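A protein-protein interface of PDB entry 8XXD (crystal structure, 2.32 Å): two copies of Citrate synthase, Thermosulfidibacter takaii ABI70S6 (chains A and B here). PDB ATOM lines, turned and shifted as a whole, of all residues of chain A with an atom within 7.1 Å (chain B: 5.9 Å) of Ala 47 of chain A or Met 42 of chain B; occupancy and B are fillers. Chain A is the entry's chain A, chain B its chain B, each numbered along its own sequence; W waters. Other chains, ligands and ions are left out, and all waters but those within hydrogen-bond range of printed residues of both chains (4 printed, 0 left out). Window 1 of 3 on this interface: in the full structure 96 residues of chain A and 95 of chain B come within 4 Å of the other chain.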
ATOM      1  N   THR A  30      16.582  -5.865 -19.309  1.00  0.00           N
ATOM      2  CA  THR A  30      17.331  -6.961 -18.708  1.00  0.00           C
ATOM      3  C   THR A  30      16.390  -7.902 -17.974  1.00  0.00           C
ATOM      4  O   THR A  30      16.667  -9.093 -17.870  1.00  0.00           O
ATOM      5  CB  THR A  30      18.407  -6.475 -17.715  1.00  0.00           C
ATOM      6  OG1 THR A  30      17.821  -5.620 -16.731  1.00  0.00           O
ATOM      7  CG2 THR A  30      19.541  -5.729 -18.390  1.00  0.00           C
ATOM      8  N   MET A  31      15.311  -7.362 -17.401  1.00  0.00           N
ATOM      9  CA  MET A  31      14.481  -8.178 -16.548  1.00  0.00           C
ATOM     10  C   MET A  31      13.277  -7.347 -16.123  1.00  0.00           C
ATOM     11  O   MET A  31      13.185  -6.149 -16.423  1.00  0.00           O
ATOM     12  CB  MET A  31      15.235  -8.683 -15.307  1.00  0.00           C
ATOM     13  CG  MET A  31      15.932  -7.550 -14.483  1.00  0.00           C
ATOM     14  SD  MET A  31      16.926  -8.104 -13.037  1.00  0.00           S
ATOM     15  CE  MET A  31      15.824  -9.281 -12.247  1.00  0.00           C
ATOM     16  N   MET A  42      15.780  -5.704  -3.189  1.00  0.00           N
ATOM     17  CA  MET A  42      16.220  -5.708  -4.582  1.00  0.00           C
ATOM     18  C   MET A  42      16.894  -7.030  -4.984  1.00  0.00           C
ATOM     19  O   MET A  42      17.649  -7.036  -5.937  1.00  0.00           O
ATOM     20  CB  MET A  42      17.239  -4.596  -4.857  1.00  0.00           C
ATOM     21  CG  MET A  42      16.759  -3.183  -4.627  1.00  0.00           C
ATOM     22  SD  MET A  42      18.061  -1.955  -5.050  1.00  0.00           S
ATOM     23  CE  MET A  42      17.420  -0.473  -4.279  1.00  0.00           C
ATOM     24  N   GLY A  44      18.358  -9.906  -6.728  1.00  0.00           N
ATOM     25  CA  GLY A  44      18.368 -10.327  -8.118  1.00  0.00           C
ATOM     26  C   GLY A  44      18.314  -9.167  -9.114  1.00  0.00           C
ATOM     27  O   GLY A  44      18.592  -9.368 -10.291  1.00  0.00           O
ATOM     28  N   LEU A  45      17.927  -7.968  -8.656  1.00  0.00           N
ATOM     29  CA  LEU A  45      17.647  -6.872  -9.566  1.00  0.00           C
ATOM     30  C   LEU A  45      18.963  -6.288 -10.066  1.00  0.00           C
ATOM     31  O   LEU A  45      19.828  -5.920  -9.264  1.00  0.00           O
ATOM     32  CB  LEU A  45      16.789  -5.833  -8.840  1.00  0.00           C
ATOM     33  CG  LEU A  45      16.196  -4.726  -9.712  1.00  0.00           C
ATOM     34  CD1 LEU A  45      15.155  -5.288 -10.681  1.00  0.00           C
ATOM     35  CD2 LEU A  45      15.579  -3.624  -8.858  1.00  0.00           C
ATOM     36  N   LYS A  46      19.099  -6.204 -11.397  1.00  0.00           N
ATOM     37  CA  LYS A  46      20.300  -5.697 -12.050  1.00  0.00           C
ATOM     38  C   LYS A  46      20.294  -4.173 -12.077  1.00  0.00           C
ATOM     39  O   LYS A  46      20.006  -3.562 -13.100  1.00  0.00           O
ATOM     40  CB  LYS A  46      20.404  -6.297 -13.458  1.00  0.00           C
ATOM     41  CG  LYS A  46      20.659  -7.800 -13.474  1.00  0.00           C
ATOM     42  CD  LYS A  46      20.542  -8.405 -14.849  1.00  0.00           C
ATOM     43  CE  LYS A  46      21.081  -9.816 -14.936  1.00  0.00           C
ATOM     44  NZ  LYS A  46      20.215 -10.778 -14.219  1.00  0.00           N
ATOM     45  N   ALA A  47      20.650  -3.553 -10.950  1.00  0.00           N
ATOM     46  CA  ALA A  47      20.469  -2.114 -10.810  1.00  0.00           C
ATOM     47  C   ALA A  47      21.790  -1.340 -10.831  1.00  0.00           C
ATOM     48  O   ALA A  47      21.769  -0.114 -10.873  1.00  0.00           O
ATOM     49  CB  ALA A  47      19.697  -1.838  -9.549  1.00  0.00           C
ATOM     50  N   LEU A  48      22.926  -2.042 -10.859  1.00  0.00           N
ATOM     51  CA  LEU A  48      24.227  -1.460 -10.570  1.00  0.00           C
ATOM     52  C   LEU A  48      25.229  -1.925 -11.617  1.00  0.00           C
ATOM     53  O   LEU A  48      25.064  -3.007 -12.170  1.00  0.00           O
ATOM     54  CB  LEU A  48      24.704  -1.957  -9.195  1.00  0.00           C
ATOM     55  CG  LEU A  48      24.291  -1.139  -7.984  1.00  0.00           C
ATOM     56  CD1 LEU A  48      25.035  -1.606  -6.747  1.00  0.00           C
ATOM     57  CD2 LEU A  48      24.567   0.333  -8.228  1.00  0.00           C
ATOM     58  N   VAL A  49      26.287  -1.125 -11.811  1.00  0.00           N
ATOM     59  CA  VAL A  49      27.451  -1.479 -12.615  1.00  0.00           C
ATOM     60  C   VAL A  49      28.677  -1.667 -11.711  1.00  0.00           C
ATOM     61  O   VAL A  49      29.006  -0.786 -10.915  1.00  0.00           O
ATOM     62  CB  VAL A  49      27.715  -0.379 -13.664  1.00  0.00           C
ATOM     63  CG1 VAL A  49      29.028  -0.557 -14.390  1.00  0.00           C
ATOM     64  CG2 VAL A  49      26.582  -0.291 -14.678  1.00  0.00           C
ATOM     65  N   HIS A 246      27.962  -1.183  -2.082  1.00  0.00           N
ATOM     66  CA  HIS A 246      26.854  -0.416  -2.603  1.00  0.00           C
ATOM     67  C   HIS A 246      26.760   0.922  -1.856  1.00  0.00           C
ATOM     68  O   HIS A 246      26.507   1.966  -2.456  1.00  0.00           O
ATOM     69  CB  HIS A 246      25.621  -1.288  -2.445  1.00  0.00           C
ATOM     70  CG  HIS A 246      24.406  -0.672  -3.027  1.00  0.00           C
ATOM     71  ND1 HIS A 246      23.176  -1.203  -2.729  1.00  0.00           N
ATOM     72  CD2 HIS A 246      24.206   0.418  -3.764  1.00  0.00           C
ATOM     73  CE1 HIS A 246      22.250  -0.465  -3.338  1.00  0.00           C
ATOM     74  NE2 HIS A 246      22.858   0.537  -3.943  1.00  0.00           N
ATOM     75  N   PRO A 418      26.055   8.953 -13.134  1.00  0.00           N
ATOM     76  CA  PRO A 418      25.336   9.976 -12.392  1.00  0.00           C
ATOM     77  C   PRO A 418      24.862   9.452 -11.040  1.00  0.00           C
ATOM     78  O   PRO A 418      24.992   8.259 -10.716  1.00  0.00           O
ATOM     79  CB  PRO A 418      24.150  10.249 -13.337  1.00  0.00           C
ATOM     80  CG  PRO A 418      23.844   8.899 -13.953  1.00  0.00           C
ATOM     81  CD  PRO A 418      25.197   8.238 -14.094  1.00  0.00           C
ATOM     82  N   ILE A 419      24.240  10.370 -10.297  1.00  0.00           N
ATOM     83  CA  ILE A 419      23.775  10.134  -8.942  1.00  0.00           C
ATOM     84  C   ILE A 419      22.826   8.954  -8.950  1.00  0.00           C
ATOM     85  O   ILE A 419      22.003   8.826  -9.838  1.00  0.00           O
ATOM     86  CB  ILE A 419      23.132  11.422  -8.379  1.00  0.00           C
ATOM     87  CG1 ILE A 419      22.922  11.366  -6.867  1.00  0.00           C
ATOM     88  CG2 ILE A 419      21.843  11.779  -9.108  1.00  0.00           C
ATOM     89  CD1 ILE A 419      22.571  12.720  -6.265  1.00  0.00           C
ATOM     90  N   GLU A 420      22.914   8.132  -7.915  1.00  0.00           N
ATOM     91  CA  GLU A 420      21.964   7.055  -7.694  1.00  0.00           C
ATOM     92  C   GLU A 420      20.699   7.626  -7.037  1.00  0.00           C
ATOM     93  O   GLU A 420      20.778   8.233  -5.973  1.00  0.00           O
ATOM     94  CB  GLU A 420      22.708   5.949  -6.934  1.00  0.00           C
ATOM     95  CG  GLU A 420      21.838   4.866  -6.339  1.00  0.00           C
ATOM     96  CD  GLU A 420      22.580   3.633  -5.847  1.00  0.00           C
ATOM     97  OE1 GLU A 420      21.923   2.735  -5.304  1.00  0.00           O
ATOM     98  OE2 GLU A 420      23.816   3.573  -6.012  1.00  0.00           O
ATOM     99  N   ARG A 421      19.536   7.440  -7.687  1.00  0.00           N
ATOM    100  CA  ARG A 421      18.249   7.977  -7.252  1.00  0.00           C
ATOM    101  C   ARG A 421      17.105   7.068  -7.728  1.00  0.00           C
ATOM    102  O   ARG A 421      16.354   7.402  -8.621  1.00  0.00           O
ATOM    103  CB  ARG A 421      18.052   9.422  -7.730  1.00  0.00           C
ATOM    104  CG  ARG A 421      17.018  10.226  -6.934  1.00  0.00           C
ATOM    105  CD  ARG A 421      16.802  11.680  -7.381  1.00  0.00           C
ATOM    106  NE  ARG A 421      15.937  11.832  -8.566  1.00  0.00           N
ATOM    107  CZ  ARG A 421      15.832  12.917  -9.351  1.00  0.00           C
ATOM    108  NH1 ARG A 421      16.619  13.965  -9.171  1.00  0.00           N
ATOM    109  NH2 ARG A 421      14.949  12.939 -10.343  1.00  0.00           N
ATOM    110  N   PRO A 422      16.872   5.902  -7.099  1.00  0.00           N
ATOM    111  CA  PRO A 422      15.733   5.069  -7.431  1.00  0.00           C
ATOM    112  C   PRO A 422      14.465   5.726  -6.908  1.00  0.00           C
ATOM    113  O   PRO A 422      14.508   6.737  -6.218  1.00  0.00           O
ATOM    114  CB  PRO A 422      15.962   3.721  -6.727  1.00  0.00           C
ATOM    115  CG  PRO A 422      17.078   3.967  -5.723  1.00  0.00           C
ATOM    116  CD  PRO A 422      17.631   5.363  -5.965  1.00  0.00           C
ATOM    117  N   LYS A 423      13.347   5.139  -7.313  1.00  0.00           N
ATOM    118  CA  LYS A 423      12.025   5.558  -6.908  1.00  0.00           C
ATOM    119  C   LYS A 423      11.563   4.611  -5.808  1.00  0.00           C
ATOM    120  O   LYS A 423      11.712   3.384  -5.911  1.00  0.00           O
ATOM    121  CB  LYS A 423      11.122   5.537  -8.143  1.00  0.00           C
ATOM    122  CG  LYS A 423       9.655   5.842  -7.899  1.00  0.00           C
ATOM    123  CD  LYS A 423       9.437   7.213  -7.326  1.00  0.00           C
ATOM    124  CE  LYS A 423       7.981   7.521  -7.066  1.00  0.00           C
ATOM    125  NZ  LYS A 423       7.810   8.970  -6.806  1.00  0.00           N
ATOM    126  N   CYS B  33      13.285  -3.288 -16.098  1.00  0.00           N
ATOM    127  CA  CYS B  33      14.643  -2.925 -15.745  1.00  0.00           C
ATOM    128  C   CYS B  33      15.492  -2.942 -17.019  1.00  0.00           C
ATOM    129  O   CYS B  33      15.436  -3.913 -17.771  1.00  0.00           O
ATOM    130  CB  CYS B  33      15.156  -3.919 -14.706  1.00  0.00           C
ATOM    131  SG  CYS B  33      16.717  -3.438 -13.920  1.00  0.00           S
ATOM    132  N   GLY B  36      19.938   1.098 -19.147  1.00  0.00           N
ATOM    133  CA  GLY B  36      20.027   2.515 -18.838  1.00  0.00           C
ATOM    134  C   GLY B  36      19.845   2.771 -17.346  1.00  0.00           C
ATOM    135  O   GLY B  36      20.383   3.753 -16.838  1.00  0.00           O
ATOM    136  N   HIS B  37      19.065   1.903 -16.676  1.00  0.00           N
ATOM    137  CA  HIS B  37      18.917   1.952 -15.231  1.00  0.00           C
ATOM    138  C   HIS B  37      20.264   1.661 -14.544  1.00  0.00           C
ATOM    139  O   HIS B  37      20.719   2.411 -13.676  1.00  0.00           O
ATOM    140  CB  HIS B  37      17.861   0.945 -14.763  1.00  0.00           C
ATOM    141  CG  HIS B  37      16.459   1.334 -15.073  1.00  0.00           C
ATOM    142  ND1 HIS B  37      15.929   2.512 -14.584  1.00  0.00           N
ATOM    143  CD2 HIS B  37      15.482   0.771 -15.780  1.00  0.00           C
ATOM    144  CE1 HIS B  37      14.682   2.643 -14.994  1.00  0.00           C
ATOM    145  NE2 HIS B  37      14.390   1.607 -15.736  1.00  0.00           N
ATOM    146  N   ALA B  38      20.931   0.579 -14.969  1.00  0.00           N
ATOM    147  CA  ALA B  38      22.162   0.130 -14.340  1.00  0.00           C
ATOM    148  C   ALA B  38      23.268   1.166 -14.458  1.00  0.00           C
ATOM    149  O   ALA B  38      24.056   1.296 -13.524  1.00  0.00           O
ATOM    150  CB  ALA B  38      22.588  -1.180 -14.920  1.00  0.00           C
ATOM    151  N   TYR B  39      23.344   1.862 -15.604  1.00  0.00           N
ATOM    152  CA  TYR B  39      24.391   2.840 -15.848  1.00  0.00           C
ATOM    153  C   TYR B  39      23.898   4.233 -15.515  1.00  0.00           C
ATOM    154  O   TYR B  39      24.639   5.184 -15.704  1.00  0.00           O
ATOM    155  CB  TYR B  39      24.850   2.845 -17.317  1.00  0.00           C
ATOM    156  CG  TYR B  39      25.735   1.683 -17.704  1.00  0.00           C
ATOM    157  CD1 TYR B  39      25.211   0.473 -18.127  1.00  0.00           C
ATOM    158  CD2 TYR B  39      27.104   1.779 -17.596  1.00  0.00           C
ATOM    159  CE1 TYR B  39      26.027  -0.602 -18.435  1.00  0.00           C
ATOM    160  CE2 TYR B  39      27.935   0.715 -17.904  1.00  0.00           C
ATOM    161  CZ  TYR B  39      27.401  -0.480 -18.332  1.00  0.00           C
ATOM    162  OH  TYR B  39      28.269  -1.512 -18.624  1.00  0.00           O
ATOM    163  N   GLY B  40      22.650   4.345 -15.035  1.00  0.00           N
ATOM    164  CA  GLY B  40      21.985   5.634 -14.976  1.00  0.00           C
ATOM    165  C   GLY B  40      21.446   5.956 -13.592  1.00  0.00           C
ATOM    166  O   GLY B  40      20.508   6.737 -13.448  1.00  0.00           O
ATOM    167  N   GLY B  41      22.108   5.391 -12.591  1.00  0.00           N
ATOM    168  CA  GLY B  41      21.781   5.661 -11.209  1.00  0.00           C
ATOM    169  C   GLY B  41      20.355   5.257 -10.858  1.00  0.00           C
ATOM    170  O   GLY B  41      19.730   5.911 -10.019  1.00  0.00           O
ATOM    171  N   MET B  42      19.848   4.211 -11.524  1.00  0.00           N
ATOM    172  CA  MET B  42      18.576   3.596 -11.187  1.00  0.00           C
ATOM    173  C   MET B  42      17.417   4.577 -11.339  1.00  0.00           C
ATOM    174  O   MET B  42      16.383   4.372 -10.686  1.00  0.00           O
ATOM    175  CB  MET B  42      18.566   3.142  -9.721  1.00  0.00           C
ATOM    176  CG  MET B  42      19.458   1.990  -9.380  1.00  0.00           C
ATOM    177  SD  MET B  42      19.119   1.451  -7.682  1.00  0.00           S
ATOM    178  CE  MET B  42      20.702   0.724  -7.283  1.00  0.00           C
ATOM    179  N   ARG B  43      17.573   5.643 -12.135  1.00  0.00           N
ATOM    180  CA  ARG B  43      16.551   6.689 -12.174  1.00  0.00           C
ATOM    181  C   ARG B  43      15.213   6.092 -12.608  1.00  0.00           C
ATOM    182  O   ARG B  43      15.114   5.522 -13.682  1.00  0.00           O
ATOM    183  CB  ARG B  43      16.911   7.801 -13.161  1.00  0.00           C
ATOM    184  CG  ARG B  43      15.985   9.014 -13.140  1.00  0.00           C
ATOM    185  CD  ARG B  43      16.263  10.088 -12.079  1.00  0.00           C
ATOM    186  NE  ARG B  43      17.612  10.676 -12.125  1.00  0.00           N
ATOM    187  CZ  ARG B  43      18.714  10.121 -11.607  1.00  0.00           C
ATOM    188  NH1 ARG B  43      18.621   9.107 -10.760  1.00  0.00           N
ATOM    189  NH2 ARG B  43      19.913  10.591 -11.915  1.00  0.00           N
ATOM    190  N   GLY B  44      14.190   6.213 -11.756  1.00  0.00           N
ATOM    191  CA  GLY B  44      12.847   5.766 -12.082  1.00  0.00           C
ATOM    192  C   GLY B  44      12.575   4.323 -11.666  1.00  0.00           C
ATOM    193  O   GLY B  44      11.434   3.886 -11.733  1.00  0.00           O
ATOM    194  N   LEU B  45      13.601   3.577 -11.223  1.00  0.00           N
ATOM    195  CA  LEU B  45      13.429   2.152 -10.963  1.00  0.00           C
ATOM    196  C   LEU B  45      12.786   1.935  -9.585  1.00  0.00           C
ATOM    197  O   LEU B  45      13.279   2.373  -8.552  1.00  0.00           O
ATOM    198  CB  LEU B  45      14.782   1.448 -11.120  1.00  0.00           C
ATOM    199  CG  LEU B  45      14.767  -0.081 -11.016  1.00  0.00           C
ATOM    200  CD1 LEU B  45      14.039  -0.709 -12.184  1.00  0.00           C
ATOM    201  CD2 LEU B  45      16.175  -0.643 -10.938  1.00  0.00           C
ATOM    202  N   LYS B  46      11.656   1.238  -9.550  1.00  0.00           N
ATOM    203  CA  LYS B  46      10.872   1.197  -8.337  1.00  0.00           C
ATOM    204  C   LYS B  46      11.442   0.097  -7.450  1.00  0.00           C
ATOM    205  O   LYS B  46      10.857  -0.974  -7.325  1.00  0.00           O
ATOM    206  CB  LYS B  46       9.399   0.997  -8.693  1.00  0.00           C
ATOM    207  CG  LYS B  46       8.764   2.136  -9.477  1.00  0.00           C
ATOM    208  CD  LYS B  46       7.278   1.917  -9.718  1.00  0.00           C
ATOM    209  CE  LYS B  46       6.794   2.443 -11.054  1.00  0.00           C
ATOM    210  NZ  LYS B  46       6.016   3.689 -10.924  1.00  0.00           N
ATOM    211  N   ALA B  47      12.581   0.380  -6.808  1.00  0.00           N
ATOM    212  CA  ALA B  47      13.368  -0.660  -6.155  1.00  0.00           C
ATOM    213  C   ALA B  47      13.304  -0.622  -4.624  1.00  0.00           C
ATOM    214  O   ALA B  47      14.045  -1.366  -3.985  1.00  0.00           O
ATOM    215  CB  ALA B  47      14.789  -0.525  -6.626  1.00  0.00           C
ATOM    216  N   HIS B 246      18.125   6.742   1.183  1.00  0.00           N
ATOM    217  CA  HIS B 246      18.455   5.409   0.706  1.00  0.00           C
ATOM    218  C   HIS B 246      19.678   4.886   1.493  1.00  0.00           C
ATOM    219  O   HIS B 246      19.672   3.768   2.032  1.00  0.00           O
ATOM    220  CB  HIS B 246      18.612   5.518  -0.822  1.00  0.00           C
ATOM    221  CG  HIS B 246      18.891   4.242  -1.520  1.00  0.00           C
ATOM    222  ND1 HIS B 246      19.515   4.208  -2.748  1.00  0.00           N
ATOM    223  CD2 HIS B 246      18.713   2.979  -1.126  1.00  0.00           C
ATOM    224  CE1 HIS B 246      19.704   2.931  -3.070  1.00  0.00           C
ATOM    225  NE2 HIS B 246      19.182   2.175  -2.123  1.00  0.00           N
ATOM    226  N   PRO B 422      21.095  -5.836  -4.249  1.00  0.00           N
ATOM    227  CA  PRO B 422      20.979  -5.888  -5.699  1.00  0.00           C
ATOM    228  C   PRO B 422      22.122  -6.639  -6.379  1.00  0.00           C
ATOM    229  O   PRO B 422      23.144  -6.905  -5.766  1.00  0.00           O
ATOM    230  CB  PRO B 422      21.028  -4.408  -6.126  1.00  0.00           C
ATOM    231  CG  PRO B 422      21.754  -3.722  -5.002  1.00  0.00           C
ATOM    232  CD  PRO B 422      21.359  -4.480  -3.748  1.00  0.00           C
ATOM    233  N   LYS B 423      21.926  -6.955  -7.664  1.00  0.00           N
ATOM    234  CA  LYS B 423      22.927  -7.573  -8.509  1.00  0.00           C
ATOM    235  C   LYS B 423      23.624  -6.484  -9.324  1.00  0.00           C
ATOM    236  O   LYS B 423      22.953  -5.651  -9.894  1.00  0.00           O
ATOM    237  CB  LYS B 423      22.222  -8.566  -9.441  1.00  0.00           C
ATOM    238  CG  LYS B 423      23.122  -9.362 -10.383  1.00  0.00           C
ATOM    239  CD  LYS B 423      24.088 -10.273  -9.655  1.00  0.00           C
ATOM    240  CE  LYS B 423      25.193 -10.810 -10.542  1.00  0.00           C
ATOM    241  NZ  LYS B 423      26.003 -11.797  -9.796  1.00  0.00           N
ATOM    242  N   SER B 424      24.957  -6.477  -9.384  1.00  0.00           N
ATOM    243  CA  SER B 424      25.655  -5.577 -10.284  1.00  0.00           C
ATOM    244  C   SER B 424      25.949  -6.352 -11.564  1.00  0.00           C
ATOM    245  O   SER B 424      25.907  -7.568 -11.537  1.00  0.00           O
ATOM    246  CB  SER B 424      26.925  -5.003  -9.652  1.00  0.00           C
ATOM    247  OG  SER B 424      27.883  -6.014  -9.398  1.00  0.00           O
ATOM    248  N   ILE B 425      26.245  -5.625 -12.656  1.00  0.00           N
ATOM    249  CA  ILE B 425      26.573  -6.198 -13.956  1.00  0.00           C
ATOM    250  C   ILE B 425      27.893  -5.598 -14.443  1.00  0.00           C
ATOM    251  O   ILE B 425      28.276  -4.488 -14.059  1.00  0.00           O
ATOM    252  CB  ILE B 425      25.428  -5.972 -14.979  1.00  0.00           C
ATOM    253  CG1 ILE B 425      25.227  -4.499 -15.348  1.00  0.00           C
ATOM    254  CG2 ILE B 425      24.122  -6.590 -14.497  1.00  0.00           C
ATOM    255  CD1 ILE B 425      23.999  -4.248 -16.237  1.00  0.00           C
HETATM  256  O   HOH W   1      13.917   8.012  -9.500  1.00  0.00           O
HETATM  257  O   HOH W   2      19.755   6.769  -3.656  1.00  0.00           O
HETATM  258  O   HOH W   3      22.790   2.360 -10.784  1.00  0.00           O
HETATM  259  O   HOH W   4      19.780  -3.565 -15.848  1.00  0.00           O
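Printed residues of chain B that touch a printed residue of chain A: Cys 33, His 37, Ala 38, Tyr 39, Gly 40, Gly 41, Met 42, Arg 43, Gly 44, Leu 45, Lys 46, Ala 47, His 246, Pro 422, Lys 423, Ser 424 and Ile 425. Hydrophobic or aromatic side chains of chain B that line the printed part of chain A: Ala 38, Tyr 39, Met 42, Leu 45, Ala 47, His 246, Pro 422 and Ile 425. Along chain B the printed residues that touch a printed residue of chain A span positions 33 to 425. Printed residues of chain A that touch a printed residue of chain B: Thr 30, Met 31, Met 42, Gly 44, Leu 45, Lys 46, Ala 47, Leu 48, Val 49, His 246, Pro 418, Ile 419, Glu 420, Arg 421, Pro 422 and Lys 423. Hydrophobic or aromatic side chains of chain A that line the printed part of chain B: Met 31, Met 42, Leu 45, Ala 47, Leu 48, Val 49, His 246, Pro 418, Ile 419 and Pro 422. Among the printed residues, 47 pairs touch across the chains. Among the printed residues, no Asp or Glu carboxylate lies within 4 Å of a Lys or Arg side-chain nitrogen of the other chain.
Water W1 bridges O of Arg 421 of chain A (2.7 Å) and N of Gly 44 of chain B (2.9 Å). Water W3 lies within hydrogen-bond range of O of Ala 47 of chain A (2.7 Å) and O of Ala 38 of chain B (3.2 Å). Water W2 lies within hydrogen-bond range of a ring nitrogen (ND1) of His 246 of chain B (2.7 Å) and the backbone carbonyl oxygen (O) of Glu 420 of chain A (2.9 Å). Water W4 lies within hydrogen-bond range of O of Lys 46 of chain A (2.8 Å), OG1 of Thr 30 of chain A (3.0 Å) and SG of Cys 33 of chain B (3.6 Å).
Of the printed residues of chain B, Leu 45 of chain A touches Leu 45, Ala 47, Pro 422 and Lys 423. Ala 47 of chain A touches five residues of chain B. Of the printed residues of chain B, Leu 48 of chain A touches Ala 38 (3.9 Å), Met 42 (3.998 Å), Lys 423 (3.7 Å), Ser 424 (3.2 Å) and Ile 425 (2.9 Å). Of the printed residues of chain B, Glu 420 of chain A touches Gly 41 (3.4 Å), Met 42 (3.1 Å) and His 246 (3.2 Å). Gly 36 of chain B touches none of the printed residues of chain A. Of the printed residues of chain A, Tyr 39 of chain B touches Val 49 (3.6 Å) and Pro 418 (3.5 Å). Printed residues of chain A within 4 Å of Gly 41 of chain B: Ile 419 (3.5 Å), Glu 420 (3.4 Å) and Arg 421 (2.8 Å). Of the printed residues of chain A, Met 42 of chain B touches Ala 47 (3.5 Å), Leu 48 (3.998 Å), His 246 (3.98 Å), Glu 420 (3.1 Å), Arg 421 (3.7 Å) and Pro 422 (3.4 Å). Of the printed residues of chain A, Gly 44 of chain B touches Arg 421 (3.99 Å) and Lys 423 (3.96 Å). The nearest residue of chain B that does not touch Ala 47 of chain A is Pro 422 of chain B (4.5 Å). The nearest printed residue of chain A that does not touch Met 42 of chain B is Met 42 of chain A (4.3 Å). The nearest printed residue of chain A that does not touch Lys 423 of chain B is Met 42 of chain A (4.6 Å).
The backbone NH (N) of Thr 30 of chain A sits at hydrogen-bond distance from the backbone carbonyl oxygen (O) of Cys 33 of chain B, at 2.7 Å. N of Ile 425 of chain B lies within hydrogen-bond range of O of Leu 48 of chain A (2.9 Å). The backbone NH (N) of Lys 423 of chain A is in hydrogen-bond range of the backbone carbonyl oxygen (O) of Leu 45 of chain B, 3.0 Å away. O of Ile 419 of chain A lies within hydrogen-bond range of NH2 of Arg 43 of chain B (3.4 Å). The backbone NH of Arg 421 of chain A sits at hydrogen-bond distance from the backbone carbonyl oxygen of Gly 41 of chain B (2.8 Å). The backbone carbonyl oxygen (O) of Met 31 of chain A is in hydrogen-bond range of the backbone NH (N) of Cys 33 of chain B (2.9 Å). The backbone carbonyl oxygen (O) of Lys 423 of chain A lies within hydrogen-bond range of the backbone NH (N) of Ala 47 of chain B (3.3 Å). N of Ala 47 of chain A sits at hydrogen-bond distance from O of Lys 423 of chain B, 3.3 Å away. The side-chain sulfur of Cys 33 of chain B is in hydrogen-bond range of the backbone carbonyl oxygen of Lys 46 of chain A (3.4 Å). The backbone carbonyl oxygen (O) of Leu 45 of chain A is in hydrogen-bond range of the backbone NH (N) of Lys 423 of chain B, 2.8 Å away.
Lys 423 of chain B touches Gly 44 of chain A. Lys 46 of chain A touches Ile 425 of chain B. Ala 47 of chain A touches His 37 of chain B. Ser 424 of chain B touches Leu 48 of chain A. CA of Val 49 of chain A touches O of Ile 425 of chain B (3.4 Å). NE2 of His 246 of chain A touches CE of Met 42 of chain B (3.98 Å). CG of Pro 422 of chain B touches ND1 of His 246 of chain A, at 3.7 Å. Gly 41 of chain B touches Ile 419 of chain A (CA to O, 3.5 Å). OE1 of Glu 420 of chain A touches CE of Met 42 of chain B, at 3.1 Å. Arg 421 of chain A touches Gly 44 of chain B.
Met 42 of chain A touches Ala 47 of chain B, and with the chains exchanged Ala 47 of chain A touches Met 42 of chain B. Met 42 of chain A touches Pro 422 of chain B, and with the chains exchanged Pro 422 of chain A touches Met 42 of chain B. Leu 45 of chain A touches Lys 423 of chain B, and with the chains exchanged Lys 423 of chain A touches Leu 45 of chain B. His 246 of chain A touches Pro 422 of chain B, and with the chains exchanged Pro 422 of chain A touches His 246 of chain B. Positions printed for both chains: 42, 44, 45, 46, 47, 246, 422 and 423.
The backbone carbonyl oxygen (O) of Gly 41 of chain B lies within hydrogen-bond range of the guanidinium group (NH1) of Arg 43 of chain B (3.5 Å). A ring nitrogen (NE2) of His 246 of chain A sits at hydrogen-bond distance from the side-chain carboxylate of Glu 420 of chain A, at 2.7 Å. SD of Met 31 of chain A sits at hydrogen-bond distance from N of Lys 46 of chain A (3.3 Å). The backbone NH (N) of Met 42 of chain B is in hydrogen-bond range of the backbone carbonyl oxygen (O) of His 37 of chain B (2.9 Å). The backbone carbonyl oxygen of Arg 43 of chain B sits close to a ring nitrogen (ND1) of His 37 of chain B (3.2 Å).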
